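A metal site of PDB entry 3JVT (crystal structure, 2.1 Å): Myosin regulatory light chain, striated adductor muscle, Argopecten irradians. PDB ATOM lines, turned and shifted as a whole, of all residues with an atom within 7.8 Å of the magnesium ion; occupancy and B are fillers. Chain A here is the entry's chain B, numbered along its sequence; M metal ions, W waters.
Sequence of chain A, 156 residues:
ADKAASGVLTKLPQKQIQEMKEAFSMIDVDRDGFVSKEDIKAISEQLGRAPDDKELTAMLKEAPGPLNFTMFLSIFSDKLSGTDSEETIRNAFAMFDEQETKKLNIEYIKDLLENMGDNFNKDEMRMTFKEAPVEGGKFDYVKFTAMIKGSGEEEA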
ATOM      1  N   PHE A  24      -0.073 -30.385  34.288  1.00  0.00           N
ATOM      2  CA  PHE A  24      -0.265 -29.652  33.052  1.00  0.00           C
ATOM      3  C   PHE A  24      -0.490 -28.184  33.347  1.00  0.00           C
ATOM      4  O   PHE A  24       0.086 -27.321  32.695  1.00  0.00           O
ATOM      5  CB  PHE A  24      -1.462 -30.173  32.266  1.00  0.00           C
ATOM      6  CG  PHE A  24      -1.688 -29.431  30.979  1.00  0.00           C
ATOM      7  CD1 PHE A  24      -1.118 -29.882  29.797  1.00  0.00           C
ATOM      8  CD2 PHE A  24      -2.399 -28.228  30.977  1.00  0.00           C
ATOM      9  CE1 PHE A  24      -1.235 -29.139  28.618  1.00  0.00           C
ATOM     10  CE2 PHE A  24      -2.532 -27.478  29.813  1.00  0.00           C
ATOM     11  CZ  PHE A  24      -1.953 -27.935  28.627  1.00  0.00           C
ATOM     12  N   SER A  25      -1.348 -27.912  34.322  1.00  0.00           N
ATOM     13  CA  SER A  25      -1.658 -26.529  34.690  1.00  0.00           C
ATOM     14  C   SER A  25      -0.402 -25.793  35.123  1.00  0.00           C
ATOM     15  O   SER A  25      -0.183 -24.653  34.719  1.00  0.00           O
ATOM     16  CB  SER A  25      -2.740 -26.478  35.779  1.00  0.00           C
ATOM     17  OG  SER A  25      -4.027 -26.748  35.237  1.00  0.00           O
ATOM     18  N   ILE A  27       2.821 -26.639  34.463  1.00  0.00           N
ATOM     19  CA  ILE A  27       3.700 -26.635  33.282  1.00  0.00           C
ATOM     20  C   ILE A  27       3.348 -25.502  32.302  1.00  0.00           C
ATOM     21  O   ILE A  27       4.233 -24.878  31.714  1.00  0.00           O
ATOM     22  CB  ILE A  27       3.647 -28.001  32.553  1.00  0.00           C
ATOM     23  CG1 ILE A  27       4.282 -29.077  33.435  1.00  0.00           C
ATOM     24  CG2 ILE A  27       4.364 -27.907  31.218  1.00  0.00           C
ATOM     25  CD1 ILE A  27       4.192 -30.489  32.850  1.00  0.00           C
ATOM     26  N   ASP A  28       2.048 -25.254  32.156  1.00  0.00           N
ATOM     27  CA  ASP A  28       1.553 -24.205  31.261  1.00  0.00           C
ATOM     28  C   ASP A  28       1.631 -22.867  32.009  1.00  0.00           C
ATOM     29  O   ASP A  28       0.624 -22.304  32.437  1.00  0.00           O
ATOM     30  CB  ASP A  28       0.112 -24.532  30.827  1.00  0.00           C
ATOM     31  CG  ASP A  28      -0.602 -23.377  30.158  1.00  0.00           C
ATOM     32  OD1 ASP A  28       0.067 -22.495  29.600  1.00  0.00           O
ATOM     33  OD2 ASP A  28      -1.834 -23.369  30.189  1.00  0.00           O
ATOM     34  N   VAL A  29       2.873 -22.387  32.152  1.00  0.00           N
ATOM     35  CA  VAL A  29       3.208 -21.128  32.818  1.00  0.00           C
ATOM     36  C   VAL A  29       2.300 -19.942  32.536  1.00  0.00           C
ATOM     37  O   VAL A  29       1.692 -19.384  33.450  1.00  0.00           O
ATOM     38  CB  VAL A  29       4.694 -20.703  32.506  1.00  0.00           C
ATOM     39  CG1 VAL A  29       4.945 -19.295  33.020  1.00  0.00           C
ATOM     40  CG2 VAL A  29       5.651 -21.694  33.158  1.00  0.00           C
ATOM     41  N   ASP A  30       2.193 -19.549  31.268  1.00  0.00           N
ATOM     42  CA  ASP A  30       1.358 -18.412  30.931  1.00  0.00           C
ATOM     43  C   ASP A  30      -0.136 -18.635  31.136  1.00  0.00           C
ATOM     44  O   ASP A  30      -0.948 -17.745  30.886  1.00  0.00           O
ATOM     45  CB  ASP A  30       1.653 -17.918  29.494  1.00  0.00           C
ATOM     46  CG  ASP A  30       1.560 -18.996  28.457  1.00  0.00           C
ATOM     47  OD1 ASP A  30       2.130 -18.806  27.363  1.00  0.00           O
ATOM     48  OD2 ASP A  30       0.905 -20.027  28.707  1.00  0.00           O
ATOM     49  N   ARG A  31      -0.494 -19.830  31.615  1.00  0.00           N
ATOM     50  CA  ARG A  31      -1.891 -20.158  31.882  1.00  0.00           C
ATOM     51  C   ARG A  31      -2.837 -19.747  30.764  1.00  0.00           C
ATOM     52  O   ARG A  31      -3.775 -18.982  30.974  1.00  0.00           O
ATOM     53  CB  ARG A  31      -2.316 -19.513  33.193  1.00  0.00           C
ATOM     54  CG  ARG A  31      -1.723 -20.157  34.442  1.00  0.00           C
ATOM     55  CD  ARG A  31      -2.810 -20.208  35.495  1.00  0.00           C
ATOM     56  NE  ARG A  31      -3.789 -19.152  35.267  1.00  0.00           N
ATOM     57  CZ  ARG A  31      -4.985 -19.083  35.839  1.00  0.00           C
ATOM     58  NH1 ARG A  31      -5.361 -20.020  36.696  1.00  0.00           N
ATOM     59  NH2 ARG A  31      -5.794 -18.091  35.536  1.00  0.00           N
ATOM     60  N   ASP A  32      -2.575 -20.283  29.569  1.00  0.00           N
ATOM     61  CA  ASP A  32      -3.379 -20.006  28.400  1.00  0.00           C
ATOM     62  C   ASP A  32      -3.987 -21.300  27.854  1.00  0.00           C
ATOM     63  O   ASP A  32      -4.759 -21.275  26.890  1.00  0.00           O
ATOM     64  CB  ASP A  32      -2.488 -19.354  27.332  1.00  0.00           C
ATOM     65  CG  ASP A  32      -1.594 -20.344  26.628  1.00  0.00           C
ATOM     66  OD1 ASP A  32      -1.003 -21.191  27.316  1.00  0.00           O
ATOM     67  OD2 ASP A  32      -1.473 -20.271  25.389  1.00  0.00           O
ATOM     68  N   GLY A  33      -3.632 -22.429  28.474  1.00  0.00           N
ATOM     69  CA  GLY A  33      -4.154 -23.715  28.029  1.00  0.00           C
ATOM     70  C   GLY A  33      -3.285 -24.550  27.109  1.00  0.00           C
ATOM     71  O   GLY A  33      -3.686 -25.639  26.706  1.00  0.00           O
ATOM     72  N   PHE A  34      -2.117 -24.038  26.752  1.00  0.00           N
ATOM     73  CA  PHE A  34      -1.203 -24.751  25.875  1.00  0.00           C
ATOM     74  C   PHE A  34       0.206 -24.703  26.448  1.00  0.00           C
ATOM     75  O   PHE A  34       0.555 -23.759  27.159  1.00  0.00           O
ATOM     76  CB  PHE A  34      -1.209 -24.114  24.484  1.00  0.00           C
ATOM     77  CG  PHE A  34      -2.578 -23.979  23.883  1.00  0.00           C
ATOM     78  CD1 PHE A  34      -3.154 -25.044  23.187  1.00  0.00           C
ATOM     79  CD2 PHE A  34      -3.306 -22.806  24.043  1.00  0.00           C
ATOM     80  CE1 PHE A  34      -4.444 -24.937  22.660  1.00  0.00           C
ATOM     81  CE2 PHE A  34      -4.598 -22.686  23.522  1.00  0.00           C
ATOM     82  CZ  PHE A  34      -5.166 -23.760  22.832  1.00  0.00           C
ATOM     83  N   VAL A  35       1.026 -25.718  26.160  1.00  0.00           N
ATOM     84  CA  VAL A  35       2.389 -25.779  26.663  1.00  0.00           C
ATOM     85  C   VAL A  35       3.392 -25.509  25.544  1.00  0.00           C
ATOM     86  O   VAL A  35       3.593 -26.334  24.659  1.00  0.00           O
ATOM     87  CB  VAL A  35       2.722 -27.161  27.280  1.00  0.00           C
ATOM     88  CG1 VAL A  35       4.161 -27.184  27.744  1.00  0.00           C
ATOM     89  CG2 VAL A  35       1.782 -27.436  28.450  1.00  0.00           C
ATOM     90  N   SER A  36       3.983 -24.316  25.575  1.00  0.00           N
ATOM     91  CA  SER A  36       4.954 -23.903  24.563  1.00  0.00           C
ATOM     92  C   SER A  36       6.388 -24.062  25.065  1.00  0.00           C
ATOM     93  O   SER A  36       6.613 -24.247  26.260  1.00  0.00           O
ATOM     94  CB  SER A  36       4.713 -22.447  24.197  1.00  0.00           C
ATOM     95  OG  SER A  36       4.631 -21.651  25.363  1.00  0.00           O
ATOM     96  N   GLU A  38       8.311 -22.007  25.660  1.00  0.00           N
ATOM     97  CA  GLU A  38       8.498 -20.977  26.663  1.00  0.00           C
ATOM     98  C   GLU A  38       8.045 -21.439  28.040  1.00  0.00           C
ATOM     99  O   GLU A  38       8.720 -21.197  29.036  1.00  0.00           O
ATOM    100  CB  GLU A  38       7.769 -19.701  26.245  1.00  0.00           C
ATOM    101  CG  GLU A  38       8.280 -19.111  24.935  1.00  0.00           C
ATOM    102  CD  GLU A  38       7.664 -19.745  23.697  1.00  0.00           C
ATOM    103  OE1 GLU A  38       6.664 -19.209  23.172  1.00  0.00           O
ATOM    104  OE2 GLU A  38       8.174 -20.788  23.237  1.00  0.00           O
ATOM    105  N   ASP A  39       6.889 -22.092  28.104  1.00  0.00           N
ATOM    106  CA  ASP A  39       6.381 -22.587  29.378  1.00  0.00           C
ATOM    107  C   ASP A  39       7.332 -23.657  29.908  1.00  0.00           C
ATOM    108  O   ASP A  39       7.693 -23.637  31.094  1.00  0.00           O
ATOM    109  CB  ASP A  39       4.986 -23.204  29.242  1.00  0.00           C
ATOM    110  CG  ASP A  39       3.883 -22.174  28.993  1.00  0.00           C
ATOM    111  OD1 ASP A  39       3.869 -21.116  29.650  1.00  0.00           O
ATOM    112  OD2 ASP A  39       3.008 -22.470  28.150  1.00  0.00           O
ATOM    113  N   ILE A  40       7.744 -24.565  29.038  1.00  0.00           N
ATOM    114  CA  ILE A  40       8.619 -25.653  29.440  1.00  0.00           C
ATOM    115  C   ILE A  40       9.940 -25.165  29.979  1.00  0.00           C
ATOM    116  O   ILE A  40      10.459 -25.697  30.951  1.00  0.00           O
ATOM    117  CB  ILE A  40       8.930 -26.613  28.286  1.00  0.00           C
ATOM    118  CG1 ILE A  40       7.660 -27.118  27.628  1.00  0.00           C
ATOM    119  CG2 ILE A  40       9.705 -27.796  28.811  1.00  0.00           C
ATOM    120  CD1 ILE A  40       7.924 -28.051  26.465  1.00  0.00           C
ATOM    121  N   LEU A  67      -0.165 -28.328  21.817  1.00  0.00           N
ATOM    122  CA  LEU A  67       0.036 -29.159  22.977  1.00  0.00           C
ATOM    123  C   LEU A  67      -0.933 -28.732  24.055  1.00  0.00           C
ATOM    124  O   LEU A  67      -0.558 -28.067  25.014  1.00  0.00           O
ATOM    125  CB  LEU A  67       1.496 -29.082  23.452  1.00  0.00           C
ATOM    126  CG  LEU A  67       2.062 -30.075  24.491  1.00  0.00           C
ATOM    127  CD1 LEU A  67       1.211 -31.295  24.604  1.00  0.00           C
ATOM    128  CD2 LEU A  67       3.472 -30.457  24.084  1.00  0.00           C
HETATM  129 MG    MG M   1       0.744 -21.971  28.008  1.00  0.00          MG
HETATM  130  O   HOH W   1       1.746 -21.468  26.106  1.00  0.00           O
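The magnesium ion is bound by OD1 of Asp 28, at 1.8 Å. O of Phe 34 binds the magnesium ion (2.0 Å). The magnesium ion is bound by OD1 of Asp 32, 2.0 Å away. OD2 of Asp 30 binds the magnesium ion, at 2.1 Å. Water W1 binds the magnesium ion (2.2 Å). OD2 of Asp 39 is bound to the magnesium ion, at 2.3 Å.
Water W1 lies within hydrogen-bond range of OD1 of Asp 30 (3.0 Å) and OG of Ser 36 (3.0 Å).
Five residues have an atom within 4 Å of the magnesium ion: Asp 28, Asp 30, Asp 32, Phe 34 and Asp 39. Along chain A the residues within 4 Å of the magnesium ion span positions 28 to 39. The nearest printed residue that does not touch the magnesium ion is Val 35 (4.2 Å).
The backbone NH (N) of Arg 31 lies close to the side-chain carboxylate (OD1) of Asp 28 (3.4 Å). The backbone NH (N) of Gly 33 sits at hydrogen-bond distance from the side-chain carboxylate (OD2) of Asp 28 (2.7 Å). The backbone NH (N) of Val 29 is in hydrogen-bond range of the side-chain carboxylate (OD1) of Asp 39 (3.0 Å). The side-chain carboxylate (OD2) of Asp 39 lies close to the backbone NH (N) of Ser 36.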
